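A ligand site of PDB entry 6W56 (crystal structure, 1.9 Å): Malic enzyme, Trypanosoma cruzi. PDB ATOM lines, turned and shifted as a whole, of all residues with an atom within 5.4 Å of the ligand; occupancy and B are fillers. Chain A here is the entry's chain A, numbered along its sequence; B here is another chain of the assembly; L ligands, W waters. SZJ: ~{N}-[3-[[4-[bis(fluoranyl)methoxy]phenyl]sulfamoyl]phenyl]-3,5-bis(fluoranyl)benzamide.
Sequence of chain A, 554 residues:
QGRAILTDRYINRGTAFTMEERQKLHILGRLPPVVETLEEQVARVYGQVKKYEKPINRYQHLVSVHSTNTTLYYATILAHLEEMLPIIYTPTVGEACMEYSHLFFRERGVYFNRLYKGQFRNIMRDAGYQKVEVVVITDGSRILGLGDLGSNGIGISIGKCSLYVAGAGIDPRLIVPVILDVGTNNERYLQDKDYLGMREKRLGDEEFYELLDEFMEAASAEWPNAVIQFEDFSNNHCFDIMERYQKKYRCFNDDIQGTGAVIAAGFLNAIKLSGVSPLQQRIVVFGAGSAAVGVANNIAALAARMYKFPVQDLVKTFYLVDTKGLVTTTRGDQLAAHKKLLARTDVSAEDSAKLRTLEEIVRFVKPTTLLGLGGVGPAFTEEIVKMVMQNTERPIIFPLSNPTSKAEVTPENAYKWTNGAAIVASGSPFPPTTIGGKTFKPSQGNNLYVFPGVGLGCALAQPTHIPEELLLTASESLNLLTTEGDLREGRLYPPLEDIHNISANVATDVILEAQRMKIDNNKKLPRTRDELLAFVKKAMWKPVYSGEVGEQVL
The side-chain amide nitrogen (ND2) of Asn 12 is in hydrogen-bond range of an oxygen (O1) of the ligand (2.7 Å).
The side-chain amide nitrogen (NE2) of Gln 41 is in hydrogen-bond range of an oxygen (O3) of the ligand, 2.9 Å away.
NH2 of Arg 44 sits at hydrogen-bond distance from O3 of the ligand.
N1 of the ligand sits at hydrogen-bond distance from O of Phe 105 of chain B.
An oxygen (O3) of the ligand sits at hydrogen-bond distance from the backbone NH (N) of Thr 15 (3.2 Å).
OG1 of Thr 15 sits at hydrogen-bond distance from O3 of the ligand (3.2 Å).
The side-chain amide nitrogen of Asn 69 lies within hydrogen-bond range of an oxygen (O2) of the ligand.
An oxygen (O4) of the ligand lies close to the backbone NH (N) of Val 65, at 3.4 Å.
The guanidinium group (NE) of Arg 30 lies within hydrogen-bond range of the backbone carbonyl oxygen (O) of Gly 109 of chain B, 3.4 Å away.
OG1 of Thr 15 sits at hydrogen-bond distance from NE2 of Gln 41, at 3.3 Å.
The side-chain amide nitrogen (NE2) of Gln 41 sits at hydrogen-bond distance from the backbone carbonyl oxygen (O) of Arg 13 (2.8 Å).
NH2 of Arg 44 is in hydrogen-bond range of OG1 of Thr 15 (3.5 Å).
OG1 of Thr 15 sits at hydrogen-bond distance from OE1 of Glu 36, 2.6 Å away.
OD1 of Asn 69 lies within hydrogen-bond range of N of Leu 72.
The side-chain hydroxyl (OG1) of Thr 68 is in hydrogen-bond range of the backbone carbonyl oxygen (O) of Ser 64 (3.2 Å).
The side-chain hydroxyl of Thr 68 sits at hydrogen-bond distance from the guanidinium group of Arg 106 of chain B (2.5 Å).
A fluorine (F2) of the ligand lies close to the backbone carbonyl oxygen (O) of Leu 6 (3.2 Å).
NH2 of Arg 30 sits close to F1 of the ligand (2.4 Å).
O of His 102 of chain B sits close to F4 of the ligand (3.3 Å).
The backbone carbonyl oxygen (O) of Glu 107 of chain B lies close to a fluorine (F1) of the ligand, at 3.3 Å.
Residues that only touch the ligand: Ser 64 (3.3 Å), Arg 106 of chain B (3.3 Å), Thr 7 (3.3 Å), His 61 (3.3 Å), Thr 68 (3.4 Å), Leu 72 (3.5 Å), Gln 48 (3.6 Å), Leu 31 (3.6 Å), Gly 14 (3.7 Å) and Val 45 (3.8 Å).
Hydrophobic or aromatic side chains within 4 Å of the ligand: Leu 6, Leu 31, Val 45, His 61, Val 65, Leu 72, His 102 of chain B and Phe 105 of chain B.
Along chain A the residues within 4 Å of the ligand span positions 6 to 72.
The nearest printed residue that does not touch the ligand is Arg 108 of chain B (4.02 Å).
Water W2 lies within hydrogen-bond range of the backbone carbonyl oxygen of Arg 30, a nitrogen (N1) of the ligand and the backbone carbonyl oxygen of Phe 105 of chain B.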
ATOM      1  N   LEU A   6       9.737   4.522  10.157  1.00  0.00           N
ATOM      2  CA  LEU A   6      10.671   5.637  10.402  1.00  0.00           C
ATOM      3  C   LEU A   6      11.829   5.150  11.273  1.00  0.00           C
ATOM      4  O   LEU A   6      12.935   5.567  11.006  1.00  0.00           O
ATOM      5  CB  LEU A   6       9.919   6.775  11.089  1.00  0.00           C
ATOM      6  CG  LEU A   6       8.913   7.527  10.250  1.00  0.00           C
ATOM      7  CD1 LEU A   6       8.215   8.557  11.116  1.00  0.00           C
ATOM      8  CD2 LEU A   6       9.570   8.181   9.063  1.00  0.00           C
ATOM      9  N   THR A   7      11.548   4.281  12.252  1.00  0.00           N
ATOM     10  CA  THR A   7      12.506   3.831  13.301  1.00  0.00           C
ATOM     11  C   THR A   7      13.380   2.685  12.792  1.00  0.00           C
ATOM     12  O   THR A   7      14.324   2.324  13.484  1.00  0.00           O
ATOM     13  CB  THR A   7      11.749   3.431  14.579  1.00  0.00           C
ATOM     14  OG1 THR A   7      10.860   2.370  14.223  1.00  0.00           O
ATOM     15  CG2 THR A   7      10.963   4.581  15.143  1.00  0.00           C
ATOM     16  N   ASP A   8      13.092   2.139  11.615  1.00  0.00           N
ATOM     17  CA  ASP A   8      13.880   1.055  10.977  1.00  0.00           C
ATOM     18  C   ASP A   8      14.792   1.690   9.905  1.00  0.00           C
ATOM     19  O   ASP A   8      14.287   2.049   8.844  1.00  0.00           O
ATOM     20  CB  ASP A   8      12.972  -0.019  10.400  1.00  0.00           C
ATOM     21  CG  ASP A   8      13.751  -1.144   9.764  1.00  0.00           C
ATOM     22  OD1 ASP A   8      14.930  -0.973   9.545  1.00  0.00           O
ATOM     23  OD2 ASP A   8      13.169  -2.156   9.452  1.00  0.00           O
ATOM     24  N   ASN A  12      13.428   3.126   6.349  1.00  0.00           N
ATOM     25  CA  ASN A  12      13.170   4.590   6.451  1.00  0.00           C
ATOM     26  C   ASN A  12      13.669   5.306   5.182  1.00  0.00           C
ATOM     27  O   ASN A  12      14.835   5.165   4.780  1.00  0.00           O
ATOM     28  CB  ASN A  12      13.794   5.178   7.703  1.00  0.00           C
ATOM     29  CG  ASN A  12      13.432   6.633   7.871  1.00  0.00           C
ATOM     30  OD1 ASN A  12      12.312   7.009   7.479  1.00  0.00           O
ATOM     31  ND2 ASN A  12      14.336   7.436   8.433  1.00  0.00           N
ATOM     32  N   ARG A  13      12.826   6.170   4.646  1.00  0.00           N
ATOM     33  CA  ARG A  13      13.117   7.008   3.479  1.00  0.00           C
ATOM     34  C   ARG A  13      13.104   8.483   3.854  1.00  0.00           C
ATOM     35  O   ARG A  13      13.391   9.299   2.989  1.00  0.00           O
ATOM     36  CB  ARG A  13      12.034   6.774   2.423  1.00  0.00           C
ATOM     37  CG  ARG A  13      11.940   5.343   1.969  1.00  0.00           C
ATOM     38  CD  ARG A  13      11.094   5.271   0.706  1.00  0.00           C
ATOM     39  NE  ARG A  13      10.674   3.909   0.512  1.00  0.00           N
ATOM     40  CZ  ARG A  13      10.151   3.442  -0.612  1.00  0.00           C
ATOM     41  NH1 ARG A  13       9.954   4.260  -1.622  1.00  0.00           N
ATOM     42  NH2 ARG A  13       9.815   2.157  -0.705  1.00  0.00           N
ATOM     43  N   GLY A  14      12.714   8.798   5.079  1.00  0.00           N
ATOM     44  CA  GLY A  14      12.540  10.184   5.531  1.00  0.00           C
ATOM     45  C   GLY A  14      11.690  10.982   4.567  1.00  0.00           C
ATOM     46  O   GLY A  14      10.605  10.511   4.237  1.00  0.00           O
ATOM     47  N   THR A  15      12.154  12.160   4.172  1.00  0.00           N
ATOM     48  CA  THR A  15      11.364  13.098   3.344  1.00  0.00           C
ATOM     49  C   THR A  15      11.087  12.539   1.947  1.00  0.00           C
ATOM     50  O   THR A  15      10.318  13.212   1.216  1.00  0.00           O
ATOM     51  CB  THR A  15      12.100  14.419   3.245  1.00  0.00           C
ATOM     52  OG1 THR A  15      13.353  14.143   2.574  1.00  0.00           O
ATOM     53  CG2 THR A  15      12.227  15.072   4.588  1.00  0.00           C
ATOM     54  N   ALA A  16      11.673  11.386   1.584  1.00  0.00           N
ATOM     55  CA  ALA A  16      11.494  10.763   0.256  1.00  0.00           C
ATOM     56  C   ALA A  16      10.159  10.025   0.249  1.00  0.00           C
ATOM     57  O   ALA A  16       9.659   9.800  -0.847  1.00  0.00           O
ATOM     58  CB  ALA A  16      12.647   9.870  -0.153  1.00  0.00           C
ATOM     59  N   ARG A  30       4.702  13.218  10.952  1.00  0.00           N
ATOM     60  CA  ARG A  30       5.911  12.691  11.648  1.00  0.00           C
ATOM     61  C   ARG A  30       7.142  13.308  10.994  1.00  0.00           C
ATOM     62  O   ARG A  30       8.232  13.110  11.514  1.00  0.00           O
ATOM     63  CB  ARG A  30       6.000  11.165  11.561  1.00  0.00           C
ATOM     64  CG  ARG A  30       4.990  10.425  12.433  1.00  0.00           C
ATOM     65  CD  ARG A  30       4.966  10.775  13.936  1.00  0.00           C
ATOM     66  NE  ARG A  30       6.309  10.765  14.509  1.00  0.00           N
ATOM     67  CZ  ARG A  30       7.041   9.663  14.782  1.00  0.00           C
ATOM     68  NH1 ARG A  30       6.558   8.449  14.576  1.00  0.00           N
ATOM     69  NH2 ARG A  30       8.254   9.797  15.289  1.00  0.00           N
ATOM     70  N   LEU A  31       6.954  13.989   9.861  1.00  0.00           N
ATOM     71  CA  LEU A  31       8.076  14.532   9.026  1.00  0.00           C
ATOM     72  C   LEU A  31       7.731  15.968   8.683  1.00  0.00           C
ATOM     73  O   LEU A  31       6.555  16.331   8.601  1.00  0.00           O
ATOM     74  CB  LEU A  31       8.210  13.708   7.747  1.00  0.00           C
ATOM     75  CG  LEU A  31       8.646  12.253   7.905  1.00  0.00           C
ATOM     76  CD1 LEU A  31       8.236  11.460   6.675  1.00  0.00           C
ATOM     77  CD2 LEU A  31      10.150  12.153   8.099  1.00  0.00           C
ATOM     78  N   PRO A  32       8.736  16.834   8.425  1.00  0.00           N
ATOM     79  CA  PRO A  32       8.454  18.168   7.871  1.00  0.00           C
ATOM     80  C   PRO A  32       7.858  17.974   6.477  1.00  0.00           C
ATOM     81  O   PRO A  32       8.002  16.901   5.905  1.00  0.00           O
ATOM     82  CB  PRO A  32       9.842  18.845   7.844  1.00  0.00           C
ATOM     83  CG  PRO A  32      10.804  17.677   7.762  1.00  0.00           C
ATOM     84  CD  PRO A  32      10.170  16.538   8.527  1.00  0.00           C
ATOM     85  N   GLU A  36      11.286  15.079  -0.908  1.00  0.00           N
ATOM     86  CA  GLU A  36      12.557  15.088  -1.675  1.00  0.00           C
ATOM     87  C   GLU A  36      12.724  13.766  -2.402  1.00  0.00           C
ATOM     88  O   GLU A  36      12.192  12.732  -1.918  1.00  0.00           O
ATOM     89  CB  GLU A  36      13.757  15.296  -0.761  1.00  0.00           C
ATOM     90  CG  GLU A  36      14.006  16.727  -0.370  1.00  0.00           C
ATOM     91  CD  GLU A  36      14.943  16.905   0.812  1.00  0.00           C
ATOM     92  OE1 GLU A  36      14.756  16.211   1.836  1.00  0.00           O
ATOM     93  OE2 GLU A  36      15.891  17.739   0.703  1.00  0.00           O
ATOM     94  N   GLN A  41      18.039  14.457  -1.281  1.00  0.00           N
ATOM     95  CA  GLN A  41      18.416  14.137   0.122  1.00  0.00           C
ATOM     96  C   GLN A  41      19.936  14.041   0.197  1.00  0.00           C
ATOM     97  O   GLN A  41      20.526  14.561   1.171  1.00  0.00           O
ATOM     98  CB  GLN A  41      17.761  12.838   0.564  1.00  0.00           C
ATOM     99  CG  GLN A  41      16.244  12.874   0.653  1.00  0.00           C
ATOM    100  CD  GLN A  41      15.773  11.506   1.059  1.00  0.00           C
ATOM    101  OE1 GLN A  41      16.089  10.532   0.410  1.00  0.00           O
ATOM    102  NE2 GLN A  41      15.086  11.410   2.203  1.00  0.00           N
ATOM    103  N   ARG A  44      21.502  17.418   0.203  1.00  0.00           N
ATOM    104  CA  ARG A  44      21.212  18.060   1.495  1.00  0.00           C
ATOM    105  C   ARG A  44      22.201  17.540   2.540  1.00  0.00           C
ATOM    106  O   ARG A  44      22.839  18.365   3.227  1.00  0.00           O
ATOM    107  CB  ARG A  44      19.751  17.868   1.941  1.00  0.00           C
ATOM    108  CG  ARG A  44      19.477  18.445   3.327  1.00  0.00           C
ATOM    109  CD  ARG A  44      17.998  18.572   3.583  1.00  0.00           C
ATOM    110  NE  ARG A  44      17.280  17.339   3.296  1.00  0.00           N
ATOM    111  CZ  ARG A  44      17.258  16.229   4.022  1.00  0.00           C
ATOM    112  NH1 ARG A  44      17.943  16.168   5.135  1.00  0.00           N
ATOM    113  NH2 ARG A  44      16.467  15.221   3.678  1.00  0.00           N
ATOM    114  N   VAL A  45      22.348  16.225   2.614  1.00  0.00           N
ATOM    115  CA  VAL A  45      23.286  15.548   3.565  1.00  0.00           C
ATOM    116  C   VAL A  45      24.703  16.038   3.250  1.00  0.00           C
ATOM    117  O   VAL A  45      25.419  16.369   4.191  1.00  0.00           O
ATOM    118  CB  VAL A  45      23.191  14.022   3.549  1.00  0.00           C
ATOM    119  CG1 VAL A  45      24.294  13.382   4.386  1.00  0.00           C
ATOM    120  CG2 VAL A  45      21.846  13.514   4.029  1.00  0.00           C
ATOM    121  N   GLN A  48      25.161  19.256   4.822  1.00  0.00           N
ATOM    122  CA  GLN A  48      25.208  19.125   6.306  1.00  0.00           C
ATOM    123  C   GLN A  48      26.640  18.676   6.708  1.00  0.00           C
ATOM    124  O   GLN A  48      27.148  19.196   7.718  1.00  0.00           O
ATOM    125  CB  GLN A  48      24.144  18.131   6.790  1.00  0.00           C
ATOM    126  CG  GLN A  48      22.696  18.598   6.697  1.00  0.00           C
ATOM    127  CD  GLN A  48      21.641  17.524   6.844  1.00  0.00           C
ATOM    128  OE1 GLN A  48      20.440  17.783   6.716  1.00  0.00           O
ATOM    129  NE2 GLN A  48      22.068  16.293   7.069  1.00  0.00           N
ATOM    130  N   HIS A  61      28.686  13.189  12.020  1.00  0.00           N
ATOM    131  CA  HIS A  61      27.437  13.460  11.257  1.00  0.00           C
ATOM    132  C   HIS A  61      27.017  12.259  10.402  1.00  0.00           C
ATOM    133  O   HIS A  61      25.804  11.884  10.390  1.00  0.00           O
ATOM    134  CB  HIS A  61      27.572  14.715  10.418  1.00  0.00           C
ATOM    135  CG  HIS A  61      26.285  15.043   9.780  1.00  0.00           C
ATOM    136  ND1 HIS A  61      25.167  15.376  10.525  1.00  0.00           N
ATOM    137  CD2 HIS A  61      25.882  14.969   8.489  1.00  0.00           C
ATOM    138  CE1 HIS A  61      24.135  15.517   9.700  1.00  0.00           C
ATOM    139  NE2 HIS A  61      24.554  15.311   8.450  1.00  0.00           N
ATOM    140  N   SER A  64      25.367   9.546  12.339  1.00  0.00           N
ATOM    141  CA  SER A  64      23.942   9.789  12.681  1.00  0.00           C
ATOM    142  C   SER A  64      23.060   9.528  11.437  1.00  0.00           C
ATOM    143  O   SER A  64      21.971   9.015  11.600  1.00  0.00           O
ATOM    144  CB  SER A  64      23.680  11.171  13.259  1.00  0.00           C
ATOM    145  OG  SER A  64      24.088  12.134  12.312  1.00  0.00           O
ATOM    146  N   VAL A  65      23.536   9.826  10.220  1.00  0.00           N
ATOM    147  CA  VAL A  65      22.755   9.536   8.973  1.00  0.00           C
ATOM    148  C   VAL A  65      22.596   8.002   8.833  1.00  0.00           C
ATOM    149  O   VAL A  65      21.456   7.506   8.632  1.00  0.00           O
ATOM    150  CB  VAL A  65      23.404  10.177   7.736  1.00  0.00           C
ATOM    151  CG1 VAL A  65      22.551   9.927   6.512  1.00  0.00           C
ATOM    152  CG2 VAL A  65      23.682  11.676   7.914  1.00  0.00           C
ATOM    153  N   THR A  68      19.986   6.476  11.002  1.00  0.00           N
ATOM    154  CA  THR A  68      18.576   6.895  10.763  1.00  0.00           C
ATOM    155  C   THR A  68      18.044   6.434   9.418  1.00  0.00           C
ATOM    156  O   THR A  68      16.885   6.008   9.372  1.00  0.00           O
ATOM    157  CB  THR A  68      18.447   8.421  10.848  1.00  0.00           C
ATOM    158  OG1 THR A  68      18.802   8.718  12.203  1.00  0.00           O
ATOM    159  CG2 THR A  68      17.052   8.914  10.505  1.00  0.00           C
ATOM    160  N   ASN A  69      18.846   6.568   8.369  1.00  0.00           N
ATOM    161  CA  ASN A  69      18.474   6.277   6.962  1.00  0.00           C
ATOM    162  C   ASN A  69      19.695   5.679   6.268  1.00  0.00           C
ATOM    163  O   ASN A  69      20.536   6.436   5.747  1.00  0.00           O
ATOM    164  CB  ASN A  69      17.929   7.529   6.289  1.00  0.00           C
ATOM    165  CG  ASN A  69      17.364   7.286   4.909  1.00  0.00           C
ATOM    166  OD1 ASN A  69      17.659   6.235   4.314  1.00  0.00           O
ATOM    167  ND2 ASN A  69      16.566   8.244   4.430  1.00  0.00           N
ATOM    168  N   LEU A  72      20.121   6.338   2.541  1.00  0.00           N
ATOM    169  CA  LEU A  72      20.594   7.734   2.274  1.00  0.00           C
ATOM    170  C   LEU A  72      22.087   7.823   2.598  1.00  0.00           C
ATOM    171  O   LEU A  72      22.859   8.498   1.897  1.00  0.00           O
ATOM    172  CB  LEU A  72      19.777   8.691   3.128  1.00  0.00           C
ATOM    173  CG  LEU A  72      20.209  10.158   3.055  1.00  0.00           C
ATOM    174  CD1 LEU A  72      20.371  10.617   1.623  1.00  0.00           C
ATOM    175  CD2 LEU A  72      19.228  11.065   3.804  1.00  0.00           C
ATOM    176  N   HIS B 102      19.192  19.245  11.681  1.00  0.00           N
ATOM    177  CA  HIS B 102      19.304  17.775  11.512  1.00  0.00           C
ATOM    178  C   HIS B 102      19.461  17.066  12.865  1.00  0.00           C
ATOM    179  O   HIS B 102      19.184  15.863  12.941  1.00  0.00           O
ATOM    180  CB  HIS B 102      20.443  17.429  10.549  1.00  0.00           C
ATOM    181  CG  HIS B 102      21.780  17.845  11.036  1.00  0.00           C
ATOM    182  ND1 HIS B 102      22.353  19.047  10.675  1.00  0.00           N
ATOM    183  CD2 HIS B 102      22.620  17.262  11.916  1.00  0.00           C
ATOM    184  CE1 HIS B 102      23.541  19.166  11.282  1.00  0.00           C
ATOM    185  NE2 HIS B 102      23.717  18.062  12.038  1.00  0.00           N
ATOM    186  N   LEU B 103      19.851  17.778  13.928  1.00  0.00           N
ATOM    187  CA  LEU B 103      19.996  17.170  15.285  1.00  0.00           C
ATOM    188  C   LEU B 103      18.637  16.705  15.832  1.00  0.00           C
ATOM    189  O   LEU B 103      18.614  15.931  16.809  1.00  0.00           O
ATOM    190  CB  LEU B 103      20.657  18.209  16.192  1.00  0.00           C
ATOM    191  CG  LEU B 103      22.129  18.480  15.882  1.00  0.00           C
ATOM    192  CD1 LEU B 103      22.657  19.500  16.863  1.00  0.00           C
ATOM    193  CD2 LEU B 103      22.938  17.184  15.910  1.00  0.00           C
ATOM    194  N   PHE B 105      16.019  15.485  13.690  1.00  0.00           N
ATOM    195  CA  PHE B 105      15.319  14.649  12.669  1.00  0.00           C
ATOM    196  C   PHE B 105      14.806  13.343  13.290  1.00  0.00           C
ATOM    197  O   PHE B 105      13.712  12.900  12.937  1.00  0.00           O
ATOM    198  CB  PHE B 105      16.209  14.364  11.458  1.00  0.00           C
ATOM    199  CG  PHE B 105      16.429  15.557  10.548  1.00  0.00           C
ATOM    200  CD1 PHE B 105      15.694  16.714  10.692  1.00  0.00           C
ATOM    201  CD2 PHE B 105      17.384  15.495   9.528  1.00  0.00           C
ATOM    202  CE1 PHE B 105      15.911  17.812   9.878  1.00  0.00           C
ATOM    203  CE2 PHE B 105      17.573  16.571   8.683  1.00  0.00           C
ATOM    204  CZ  PHE B 105      16.855  17.731   8.879  1.00  0.00           C
ATOM    205  N   ARG B 106      15.598  12.718  14.150  1.00  0.00           N
ATOM    206  CA  ARG B 106      15.313  11.350  14.646  1.00  0.00           C
ATOM    207  C   ARG B 106      14.273  11.386  15.773  1.00  0.00           C
ATOM    208  O   ARG B 106      13.746  10.327  16.168  1.00  0.00           O
ATOM    209  CB  ARG B 106      16.612  10.724  15.162  1.00  0.00           C
ATOM    210  CG  ARG B 106      17.869  11.228  14.456  1.00  0.00           C
ATOM    211  CD  ARG B 106      19.113  10.410  14.779  1.00  0.00           C
ATOM    212  NE  ARG B 106      18.747   8.997  14.732  1.00  0.00           N
ATOM    213  CZ  ARG B 106      19.535   7.998  15.032  1.00  0.00           C
ATOM    214  NH1 ARG B 106      20.782   8.226  15.415  1.00  0.00           N
ATOM    215  NH2 ARG B 106      19.067   6.761  14.939  1.00  0.00           N
ATOM    216  N   GLU B 107      14.008  12.565  16.312  1.00  0.00           N
ATOM    217  CA  GLU B 107      13.172  12.681  17.536  1.00  0.00           C
ATOM    218  C   GLU B 107      11.690  12.562  17.194  1.00  0.00           C
ATOM    219  O   GLU B 107      11.261  13.063  16.149  1.00  0.00           O
ATOM    220  CB  GLU B 107      13.356  14.009  18.240  1.00  0.00           C
ATOM    221  CG  GLU B 107      14.781  14.243  18.682  1.00  0.00           C
ATOM    222  CD  GLU B 107      15.421  12.996  19.240  1.00  0.00           C
ATOM    223  OE1 GLU B 107      14.838  12.338  20.161  1.00  0.00           O
ATOM    224  OE2 GLU B 107      16.505  12.698  18.742  1.00  0.00           O
ATOM    225  N   ARG B 108      10.943  12.031  18.129  1.00  0.00           N
ATOM    226  CA  ARG B 108       9.504  11.783  17.967  1.00  0.00           C
ATOM    227  C   ARG B 108       8.831  13.117  18.215  1.00  0.00           C
ATOM    228  O   ARG B 108       8.853  13.536  19.346  1.00  0.00           O
ATOM    229  CB  ARG B 108       9.024  10.753  18.995  1.00  0.00           C
ATOM    230  CG  ARG B 108       7.803   9.980  18.535  1.00  0.00           C
ATOM    231  CD  ARG B 108       7.574   8.677  19.281  1.00  0.00           C
ATOM    232  NE  ARG B 108       6.150   8.595  19.552  1.00  0.00           N
ATOM    233  CZ  ARG B 108       5.523   7.495  19.964  1.00  0.00           C
ATOM    234  NH1 ARG B 108       6.199   6.378  20.155  1.00  0.00           N
ATOM    235  NH2 ARG B 108       4.219   7.533  20.185  1.00  0.00           N
ATOM    236  N   GLY B 109       8.239  13.706  17.187  1.00  0.00           N
ATOM    237  CA  GLY B 109       7.405  14.928  17.283  1.00  0.00           C
ATOM    238  C   GLY B 109       6.296  14.945  16.251  1.00  0.00           C
ATOM    239  O   GLY B 109       6.168  13.994  15.447  1.00  0.00           O
ATOM    240  N   LEU B 196      12.948  22.546   5.013  1.00  0.00           N
ATOM    241  CA  LEU B 196      12.033  21.404   4.811  1.00  0.00           C
ATOM    242  C   LEU B 196      10.648  21.804   5.267  1.00  0.00           C
ATOM    243  O   LEU B 196       9.769  20.962   5.210  1.00  0.00           O
ATOM    244  CB  LEU B 196      12.542  20.177   5.581  1.00  0.00           C
ATOM    245  CG  LEU B 196      13.908  19.676   5.140  1.00  0.00           C
ATOM    246  CD1 LEU B 196      14.294  18.470   5.953  1.00  0.00           C
ATOM    247  CD2 LEU B 196      13.942  19.299   3.659  1.00  0.00           C
HETATM  248  N1  SZJ L   1      13.014  11.834  10.224  1.00  0.00           N
HETATM  249  C4  SZJ L   1      13.258   8.686  12.135  1.00  0.00           C
HETATM  250  C5  SZJ L   1      12.743   9.891  11.677  1.00  0.00           C
HETATM  251  C6  SZJ L   1      11.711  10.504  12.390  1.00  0.00           C
HETATM  252  C7  SZJ L   1      13.265  10.498  10.415  1.00  0.00           C
HETATM  253  C8  SZJ L   1      13.548  12.666   9.201  1.00  0.00           C
HETATM  254  C10 SZJ L   1      13.825  14.871   8.284  1.00  0.00           C
HETATM  255  C13 SZJ L   1      14.411  12.154   8.222  1.00  0.00           C
HETATM  256  C15 SZJ L   1      18.016  11.929   8.144  1.00  0.00           C
HETATM  257  C17 SZJ L   1      20.170  12.457   9.068  1.00  0.00           C
HETATM  258  C20 SZJ L   1      21.164  13.077  11.091  1.00  0.00           C
HETATM  259  C1  SZJ L   1      11.265   9.913  13.544  1.00  0.00           C
HETATM  260  C2  SZJ L   1      11.767   8.739  14.040  1.00  0.00           C
HETATM  261  C3  SZJ L   1      12.778   8.165  13.314  1.00  0.00           C
HETATM  262  F1  SZJ L   1      10.285  10.525  14.230  1.00  0.00           F
HETATM  263  F2  SZJ L   1      13.300   7.012  13.800  1.00  0.00           F
HETATM  264  O1  SZJ L   1      13.871   9.802   9.625  1.00  0.00           O
HETATM  265  C9  SZJ L   1      13.274  14.036   9.247  1.00  0.00           C
HETATM  266  C11 SZJ L   1      14.630  14.356   7.273  1.00  0.00           C
HETATM  267  C12 SZJ L   1      14.932  13.008   7.247  1.00  0.00           C
HETATM  268  S1  SZJ L   1      15.918  12.326   5.904  1.00  0.00           S
HETATM  269  N2  SZJ L   1      17.370  12.972   6.003  1.00  0.00           N
HETATM  270  O2  SZJ L   1      16.068  10.910   6.135  1.00  0.00           O
HETATM  271  O3  SZJ L   1      15.237  12.744   4.721  1.00  0.00           O
HETATM  272  C14 SZJ L   1      18.282  12.752   7.067  1.00  0.00           C
HETATM  273  C16 SZJ L   1      18.960  11.776   9.135  1.00  0.00           C
HETATM  274  C18 SZJ L   1      20.427  13.280   7.991  1.00  0.00           C
HETATM  275  C19 SZJ L   1      19.482  13.443   6.999  1.00  0.00           C
HETATM  276  O4  SZJ L   1      21.148  12.261  10.014  1.00  0.00           O
HETATM  277  F3  SZJ L   1      21.150  14.312  10.627  1.00  0.00           F
HETATM  278  F4  SZJ L   1      20.042  12.934  11.752  1.00  0.00           F
HETATM  279  O   HOH W   1       8.751  12.741  14.261  1.00  0.00           O
HETATM  280  O   HOH W   2      10.928  13.650  11.634  1.00  0.00           O
